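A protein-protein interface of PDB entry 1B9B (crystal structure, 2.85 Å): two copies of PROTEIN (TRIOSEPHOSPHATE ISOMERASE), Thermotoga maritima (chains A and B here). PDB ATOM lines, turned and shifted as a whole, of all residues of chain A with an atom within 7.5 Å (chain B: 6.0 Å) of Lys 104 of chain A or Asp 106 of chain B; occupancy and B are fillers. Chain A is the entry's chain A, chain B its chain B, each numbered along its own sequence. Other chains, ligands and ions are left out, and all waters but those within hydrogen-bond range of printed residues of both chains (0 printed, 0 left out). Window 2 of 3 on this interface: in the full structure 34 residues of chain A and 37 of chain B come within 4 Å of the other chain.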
ATOM      1  N   SER A  97      -4.713  -7.443   1.979  1.00  0.00           N
ATOM      2  CA  SER A  97      -4.895  -6.086   2.469  1.00  0.00           C
ATOM      3  C   SER A  97      -3.633  -5.482   3.087  1.00  0.00           C
ATOM      4  O   SER A  97      -3.313  -4.316   2.865  1.00  0.00           O
ATOM      5  CB  SER A  97      -6.029  -6.079   3.493  1.00  0.00           C
ATOM      6  OG  SER A  97      -6.337  -4.761   3.904  1.00  0.00           O
ATOM      7  N   GLU A  98      -2.925  -6.276   3.877  1.00  0.00           N
ATOM      8  CA  GLU A  98      -1.705  -5.812   4.505  1.00  0.00           C
ATOM      9  C   GLU A  98      -0.690  -5.389   3.446  1.00  0.00           C
ATOM     10  O   GLU A  98      -0.041  -4.353   3.587  1.00  0.00           O
ATOM     11  CB  GLU A  98      -1.146  -6.910   5.409  1.00  0.00           C
ATOM     12  CG  GLU A  98      -1.767  -6.900   6.799  1.00  0.00           C
ATOM     13  CD  GLU A  98      -1.938  -8.283   7.391  1.00  0.00           C
ATOM     14  OE1 GLU A  98      -1.089  -9.161   7.119  1.00  0.00           O
ATOM     15  OE2 GLU A  98      -2.920  -8.483   8.141  1.00  0.00           O
ATOM     16  N   ARG A  99      -0.567  -6.178   2.379  1.00  0.00           N
ATOM     17  CA  ARG A  99       0.369  -5.861   1.295  1.00  0.00           C
ATOM     18  C   ARG A  99      -0.081  -4.614   0.519  1.00  0.00           C
ATOM     19  O   ARG A  99       0.728  -3.745   0.170  1.00  0.00           O
ATOM     20  CB  ARG A  99       0.474  -7.022   0.303  1.00  0.00           C
ATOM     21  CG  ARG A  99       0.856  -8.369   0.880  1.00  0.00           C
ATOM     22  CD  ARG A  99       2.244  -8.379   1.451  1.00  0.00           C
ATOM     23  NE  ARG A  99       3.241  -7.835   0.541  1.00  0.00           N
ATOM     24  CZ  ARG A  99       4.530  -7.729   0.850  1.00  0.00           C
ATOM     25  NH1 ARG A  99       4.968  -8.141   2.040  1.00  0.00           N
ATOM     26  NH2 ARG A  99       5.380  -7.185  -0.014  1.00  0.00           N
ATOM     27  N   ARG A 100      -1.373  -4.535   0.237  1.00  0.00           N
ATOM     28  CA  ARG A 100      -1.895  -3.399  -0.503  1.00  0.00           C
ATOM     29  C   ARG A 100      -1.651  -2.120   0.286  1.00  0.00           C
ATOM     30  O   ARG A 100      -1.067  -1.163  -0.225  1.00  0.00           O
ATOM     31  CB  ARG A 100      -3.401  -3.560  -0.754  1.00  0.00           C
ATOM     32  CG  ARG A 100      -3.783  -4.807  -1.513  1.00  0.00           C
ATOM     33  CD  ARG A 100      -5.287  -5.045  -1.476  1.00  0.00           C
ATOM     34  NE  ARG A 100      -5.930  -4.801  -2.766  1.00  0.00           N
ATOM     35  CZ  ARG A 100      -6.004  -5.690  -3.749  1.00  0.00           C
ATOM     36  NH1 ARG A 100      -5.477  -6.890  -3.600  1.00  0.00           N
ATOM     37  NH2 ARG A 100      -6.604  -5.377  -4.886  1.00  0.00           N
ATOM     38  N   ARG A 101      -2.083  -2.130   1.546  1.00  0.00           N
ATOM     39  CA  ARG A 101      -1.984  -0.962   2.410  1.00  0.00           C
ATOM     40  C   ARG A 101      -0.620  -0.622   3.001  1.00  0.00           C
ATOM     41  O   ARG A 101      -0.119   0.477   2.789  1.00  0.00           O
ATOM     42  CB  ARG A 101      -3.026  -1.069   3.523  1.00  0.00           C
ATOM     43  CG  ARG A 101      -4.433  -1.356   3.008  1.00  0.00           C
ATOM     44  CD  ARG A 101      -5.478  -0.664   3.852  1.00  0.00           C
ATOM     45  NE  ARG A 101      -5.300  -0.976   5.264  1.00  0.00           N
ATOM     46  CZ  ARG A 101      -5.697  -0.183   6.252  1.00  0.00           C
ATOM     47  NH1 ARG A 101      -6.295   0.969   5.970  1.00  0.00           N
ATOM     48  NH2 ARG A 101      -5.485  -0.533   7.516  1.00  0.00           N
ATOM     49  N   ILE A 102      -0.012  -1.539   3.738  1.00  0.00           N
ATOM     50  CA  ILE A 102       1.289  -1.240   4.323  1.00  0.00           C
ATOM     51  C   ILE A 102       2.411  -1.183   3.288  1.00  0.00           C
ATOM     52  O   ILE A 102       3.250  -0.288   3.329  1.00  0.00           O
ATOM     53  CB  ILE A 102       1.684  -2.278   5.378  1.00  0.00           C
ATOM     54  CG1 ILE A 102       0.672  -2.285   6.518  1.00  0.00           C
ATOM     55  CG2 ILE A 102       3.071  -1.975   5.905  1.00  0.00           C
ATOM     56  CD1 ILE A 102       0.841  -3.482   7.436  1.00  0.00           C
ATOM     57  N   PHE A 103       2.418  -2.130   2.355  1.00  0.00           N
ATOM     58  CA  PHE A 103       3.470  -2.186   1.353  1.00  0.00           C
ATOM     59  C   PHE A 103       3.162  -1.583  -0.007  1.00  0.00           C
ATOM     60  O   PHE A 103       3.893  -1.780  -0.984  1.00  0.00           O
ATOM     61  CB  PHE A 103       3.949  -3.618   1.247  1.00  0.00           C
ATOM     62  CG  PHE A 103       4.372  -4.164   2.561  1.00  0.00           C
ATOM     63  CD1 PHE A 103       5.502  -3.655   3.197  1.00  0.00           C
ATOM     64  CD2 PHE A 103       3.589  -5.100   3.228  1.00  0.00           C
ATOM     65  CE1 PHE A 103       5.844  -4.058   4.478  1.00  0.00           C
ATOM     66  CE2 PHE A 103       3.923  -5.515   4.519  1.00  0.00           C
ATOM     67  CZ  PHE A 103       5.057  -4.987   5.144  1.00  0.00           C
ATOM     68  N   LYS A 104       2.070  -0.841  -0.056  1.00  0.00           N
ATOM     69  CA  LYS A 104       1.692  -0.127  -1.254  1.00  0.00           C
ATOM     70  C   LYS A 104       1.707  -0.897  -2.569  1.00  0.00           C
ATOM     71  O   LYS A 104       2.221  -0.397  -3.570  1.00  0.00           O
ATOM     72  CB  LYS A 104       2.598   1.096  -1.373  1.00  0.00           C
ATOM     73  CG  LYS A 104       2.683   1.897  -0.083  1.00  0.00           C
ATOM     74  CD  LYS A 104       4.002   2.648   0.027  1.00  0.00           C
ATOM     75  CE  LYS A 104       4.239   3.159   1.450  1.00  0.00           C
ATOM     76  NZ  LYS A 104       5.568   3.825   1.624  1.00  0.00           N
ATOM     77  N   GLU A 105       1.156  -2.103  -2.582  1.00  0.00           N
ATOM     78  CA  GLU A 105       1.105  -2.860  -3.820  1.00  0.00           C
ATOM     79  C   GLU A 105      -0.189  -2.456  -4.510  1.00  0.00           C
ATOM     80  O   GLU A 105      -1.259  -2.528  -3.907  1.00  0.00           O
ATOM     81  CB  GLU A 105       1.114  -4.364  -3.547  1.00  0.00           C
ATOM     82  CG  GLU A 105       2.375  -4.857  -2.857  1.00  0.00           C
ATOM     83  CD  GLU A 105       2.539  -6.371  -2.908  1.00  0.00           C
ATOM     84  OE1 GLU A 105       1.743  -7.037  -3.605  1.00  0.00           O
ATOM     85  OE2 GLU A 105       3.472  -6.889  -2.253  1.00  0.00           O
ATOM     86  N   ASP A 106      -0.090  -2.015  -5.763  1.00  0.00           N
ATOM     87  CA  ASP A 106      -1.266  -1.590  -6.527  1.00  0.00           C
ATOM     88  C   ASP A 106      -1.841  -2.707  -7.389  1.00  0.00           C
ATOM     89  O   ASP A 106      -1.203  -3.742  -7.594  1.00  0.00           O
ATOM     90  CB  ASP A 106      -0.913  -0.407  -7.417  1.00  0.00           C
ATOM     91  CG  ASP A 106       0.164  -0.744  -8.412  1.00  0.00           C
ATOM     92  OD1 ASP A 106       1.242  -1.214  -7.985  1.00  0.00           O
ATOM     93  OD2 ASP A 106      -0.067  -0.543  -9.623  1.00  0.00           O
ATOM     94  N   ASP A 107      -3.047  -2.489  -7.903  1.00  0.00           N
ATOM     95  CA  ASP A 107      -3.704  -3.494  -8.725  1.00  0.00           C
ATOM     96  C   ASP A 107      -2.866  -4.078  -9.869  1.00  0.00           C
ATOM     97  O   ASP A 107      -2.873  -5.292 -10.068  1.00  0.00           O
ATOM     98  CB  ASP A 107      -5.026  -2.947  -9.266  1.00  0.00           C
ATOM     99  CG  ASP A 107      -6.135  -2.960  -8.223  1.00  0.00           C
ATOM    100  OD1 ASP A 107      -6.401  -4.034  -7.643  1.00  0.00           O
ATOM    101  OD2 ASP A 107      -6.753  -1.901  -7.990  1.00  0.00           O
ATOM    102  N   PHE A 109       0.431  -4.325 -10.150  1.00  0.00           N
ATOM    103  CA  PHE A 109       1.417  -5.164  -9.484  1.00  0.00           C
ATOM    104  C   PHE A 109       0.748  -6.501  -9.154  1.00  0.00           C
ATOM    105  O   PHE A 109       1.252  -7.566  -9.507  1.00  0.00           O
ATOM    106  CB  PHE A 109       1.852  -4.483  -8.192  1.00  0.00           C
ATOM    107  CG  PHE A 109       3.221  -4.877  -7.718  1.00  0.00           C
ATOM    108  CD1 PHE A 109       4.358  -4.424  -8.382  1.00  0.00           C
ATOM    109  CD2 PHE A 109       3.377  -5.667  -6.583  1.00  0.00           C
ATOM    110  CE1 PHE A 109       5.630  -4.747  -7.921  1.00  0.00           C
ATOM    111  CE2 PHE A 109       4.645  -5.998  -6.114  1.00  0.00           C
ATOM    112  CZ  PHE A 109       5.771  -5.537  -6.783  1.00  0.00           C
ATOM    113  N   ARG B 100      14.328   0.393  -2.346  1.00  0.00           N
ATOM    114  CA  ARG B 100      13.999   1.809  -2.265  1.00  0.00           C
ATOM    115  C   ARG B 100      13.252   2.272  -3.526  1.00  0.00           C
ATOM    116  O   ARG B 100      12.200   2.903  -3.437  1.00  0.00           O
ATOM    117  CB  ARG B 100      15.276   2.648  -2.067  1.00  0.00           C
ATOM    118  CG  ARG B 100      16.112   2.203  -0.876  1.00  0.00           C
ATOM    119  CD  ARG B 100      17.391   3.019  -0.688  1.00  0.00           C
ATOM    120  NE  ARG B 100      17.200   4.160   0.202  1.00  0.00           N
ATOM    121  CZ  ARG B 100      17.878   4.369   1.330  1.00  0.00           C
ATOM    122  NH1 ARG B 100      18.811   3.517   1.732  1.00  0.00           N
ATOM    123  NH2 ARG B 100      17.617   5.439   2.066  1.00  0.00           N
ATOM    124  N   PHE B 103      10.171  -1.001  -4.604  1.00  0.00           N
ATOM    125  CA  PHE B 103       9.185  -1.267  -3.555  1.00  0.00           C
ATOM    126  C   PHE B 103       8.920  -0.114  -2.594  1.00  0.00           C
ATOM    127  O   PHE B 103       8.559  -0.336  -1.440  1.00  0.00           O
ATOM    128  CB  PHE B 103       9.611  -2.511  -2.780  1.00  0.00           C
ATOM    129  CG  PHE B 103       9.797  -3.711  -3.650  1.00  0.00           C
ATOM    130  CD1 PHE B 103       8.701  -4.451  -4.078  1.00  0.00           C
ATOM    131  CD2 PHE B 103      11.056  -4.052  -4.118  1.00  0.00           C
ATOM    132  CE1 PHE B 103       8.855  -5.514  -4.966  1.00  0.00           C
ATOM    133  CE2 PHE B 103      11.222  -5.112  -5.006  1.00  0.00           C
ATOM    134  CZ  PHE B 103      10.118  -5.844  -5.432  1.00  0.00           C
ATOM    135  N   LYS B 104       9.088   1.108  -3.091  1.00  0.00           N
ATOM    136  CA  LYS B 104       8.871   2.330  -2.325  1.00  0.00           C
ATOM    137  C   LYS B 104       9.223   2.283  -0.837  1.00  0.00           C
ATOM    138  O   LYS B 104       8.464   2.747   0.012  1.00  0.00           O
ATOM    139  CB  LYS B 104       7.425   2.791  -2.489  1.00  0.00           C
ATOM    140  CG  LYS B 104       7.108   3.319  -3.876  1.00  0.00           C
ATOM    141  CD  LYS B 104       6.825   2.186  -4.841  1.00  0.00           C
ATOM    142  CE  LYS B 104       5.408   1.643  -4.665  1.00  0.00           C
ATOM    143  NZ  LYS B 104       4.370   2.644  -5.076  1.00  0.00           N
ATOM    144  N   GLU B 105      10.393   1.744  -0.532  1.00  0.00           N
ATOM    145  CA  GLU B 105      10.862   1.639   0.840  1.00  0.00           C
ATOM    146  C   GLU B 105      11.558   2.968   1.203  1.00  0.00           C
ATOM    147  O   GLU B 105      12.571   3.323   0.603  1.00  0.00           O
ATOM    148  CB  GLU B 105      11.829   0.456   0.919  1.00  0.00           C
ATOM    149  CG  GLU B 105      11.936  -0.195   2.266  1.00  0.00           C
ATOM    150  CD  GLU B 105      12.080  -1.702   2.168  1.00  0.00           C
ATOM    151  OE1 GLU B 105      11.152  -2.364   1.641  1.00  0.00           O
ATOM    152  OE2 GLU B 105      13.122  -2.221   2.622  1.00  0.00           O
ATOM    153  N   ASP B 106      11.017   3.706   2.174  1.00  0.00           N
ATOM    154  CA  ASP B 106      11.605   4.992   2.557  1.00  0.00           C
ATOM    155  C   ASP B 106      12.621   4.965   3.697  1.00  0.00           C
ATOM    156  O   ASP B 106      12.821   3.944   4.355  1.00  0.00           O
ATOM    157  CB  ASP B 106      10.503   6.018   2.876  1.00  0.00           C
ATOM    158  CG  ASP B 106       9.590   5.578   4.006  1.00  0.00           C
ATOM    159  OD1 ASP B 106      10.069   5.438   5.151  1.00  0.00           O
ATOM    160  OD2 ASP B 106       8.383   5.374   3.749  1.00  0.00           O
ATOM    161  N   ASP B 107      13.262   6.108   3.918  1.00  0.00           N
ATOM    162  CA  ASP B 107      14.273   6.250   4.953  1.00  0.00           C
ATOM    163  C   ASP B 107      13.826   5.853   6.358  1.00  0.00           C
ATOM    164  O   ASP B 107      14.504   5.087   7.036  1.00  0.00           O
ATOM    165  CB  ASP B 107      14.791   7.688   4.966  1.00  0.00           C
ATOM    166  CG  ASP B 107      15.669   8.001   3.773  1.00  0.00           C
ATOM    167  OD1 ASP B 107      16.739   7.377   3.644  1.00  0.00           O
ATOM    168  OD2 ASP B 107      15.297   8.870   2.962  1.00  0.00           O
ATOM    169  N   GLU B 108      12.693   6.384   6.799  1.00  0.00           N
ATOM    170  CA  GLU B 108      12.169   6.083   8.125  1.00  0.00           C
ATOM    171  C   GLU B 108      11.866   4.597   8.263  1.00  0.00           C
ATOM    172  O   GLU B 108      12.014   4.010   9.335  1.00  0.00           O
ATOM    173  CB  GLU B 108      10.912   6.912   8.366  1.00  0.00           C
ATOM    174  CG  GLU B 108      10.098   6.504   9.572  1.00  0.00           C
ATOM    175  CD  GLU B 108       8.816   7.311   9.688  1.00  0.00           C
ATOM    176  OE1 GLU B 108       8.661   8.302   8.933  1.00  0.00           O
ATOM    177  OE2 GLU B 108       7.967   6.955  10.536  1.00  0.00           O
ATOM    178  N   PHE B 109      11.441   3.993   7.163  1.00  0.00           N
ATOM    179  CA  PHE B 109      11.128   2.572   7.118  1.00  0.00           C
ATOM    180  C   PHE B 109      12.458   1.822   7.306  1.00  0.00           C
ATOM    181  O   PHE B 109      12.570   0.886   8.104  1.00  0.00           O
ATOM    182  CB  PHE B 109      10.518   2.260   5.749  1.00  0.00           C
ATOM    183  CG  PHE B 109       9.684   1.021   5.708  1.00  0.00           C
ATOM    184  CD1 PHE B 109      10.269  -0.231   5.654  1.00  0.00           C
ATOM    185  CD2 PHE B 109       8.302   1.109   5.700  1.00  0.00           C
ATOM    186  CE1 PHE B 109       9.489  -1.381   5.587  1.00  0.00           C
ATOM    187  CE2 PHE B 109       7.514  -0.034   5.633  1.00  0.00           C
ATOM    188  CZ  PHE B 109       8.113  -1.282   5.577  1.00  0.00           C
ATOM    189  N   ILE B 110      13.472   2.266   6.573  1.00  0.00           N
ATOM    190  CA  ILE B 110      14.792   1.662   6.622  1.00  0.00           C
ATOM    191  C   ILE B 110      15.508   1.845   7.958  1.00  0.00           C
ATOM    192  O   ILE B 110      16.219   0.938   8.405  1.00  0.00           O
ATOM    193  CB  ILE B 110      15.647   2.206   5.474  1.00  0.00           C
ATOM    194  CG1 ILE B 110      15.002   1.792   4.149  1.00  0.00           C
ATOM    195  CG2 ILE B 110      17.071   1.668   5.565  1.00  0.00           C
ATOM    196  CD1 ILE B 110      15.627   2.403   2.937  1.00  0.00           C
ATOM    197  N   ASN B 111      15.316   3.008   8.589  1.00  0.00           N
ATOM    198  CA  ASN B 111      15.914   3.312   9.894  1.00  0.00           C
ATOM    199  C   ASN B 111      15.416   2.313  10.944  1.00  0.00           C
ATOM    200  O   ASN B 111      16.182   1.844  11.792  1.00  0.00           O
ATOM    201  CB  ASN B 111      15.541   4.735  10.326  1.00  0.00           C
ATOM    202  CG  ASN B 111      16.088   5.098  11.705  1.00  0.00           C
ATOM    203  OD1 ASN B 111      15.672   4.545  12.716  1.00  0.00           O
ATOM    204  ND2 ASN B 111      17.030   6.028  11.741  1.00  0.00           N
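Hydrophobic or aromatic side chains of chain A within 4 Å of the printed part of chain B: Phe 103 and Phe 109.
Hydrophobic or aromatic side chains of chain B within 4 Å of the printed part of chain A: Phe 103 and Phe 109.
The backbone NH (N) of Lys 104 of chain A is in hydrogen-bond range of the backbone carbonyl oxygen (O) of Arg 99 of chain A (3.2 Å).
The side-chain carboxylate (OD1) of Asp 106 of chain B sits at hydrogen-bond distance from the backbone NH (N) of Glu 108 of chain B, at 3.2 Å.
The backbone NH of Phe 109 of chain B sits at hydrogen-bond distance from the side-chain carboxylate of Asp 106 of chain B (2.8 Å).
Lys 104 of chain A touches just these residues of chain B: Lys 104 and Asp 106.
Of the printed residues of chain A, Asp 106 of chain B touches Lys 104 (3.9 Å).
Of the printed residues of chain A, Lys 104 of chain B touches Lys 104 (3.5 Å).
Of the printed residues of chain B, Phe 103 of chain A touches Phe 109 (3.7 Å).
Of the printed residues of chain A, Phe 109 of chain B touches Phe 103 (3.7 Å).
Of the printed residues of chain B, Phe 109 of chain A touches Phe 103 (3.6 Å).
Of the printed residues of chain A, Phe 103 of chain B touches Phe 109.
Asp 107 of chain B touches none of the printed residues of chain A.
The nearest printed residue of chain A that does not touch Asp 106 of chain B is Ile 102 of chain A (7.7 Å).
NZ of Lys 104 of chain A is in hydrogen-bond range of O of Lys 104 of chain B (3.5 Å).
The side-chain amino group (NZ) of Lys 104 of chain A is in salt-bridge range of the side-chain carboxylate (OD2) of Asp 106 of chain B (3.9 Å).
Phe 103 of chain A touches Phe 109 of chain B, and with the chains exchanged Phe 109 of chain A touches Phe 103 of chain B.
Lys 104 of chain A touches its own counterpart, Lys 104 of chain B.
Lys 104 of chain A touches Asp 106 of chain B, but with the chains exchanged Asp 106 of chain A does not touch Lys 104 of chain B (5.8 Å).
Among the printed residues, merely in contact across the chains: Phe 109 of chain A with Phe 103 of chain B (3.6 Å) and Phe 103 of chain A with Phe 109 of chain B (3.7 Å).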
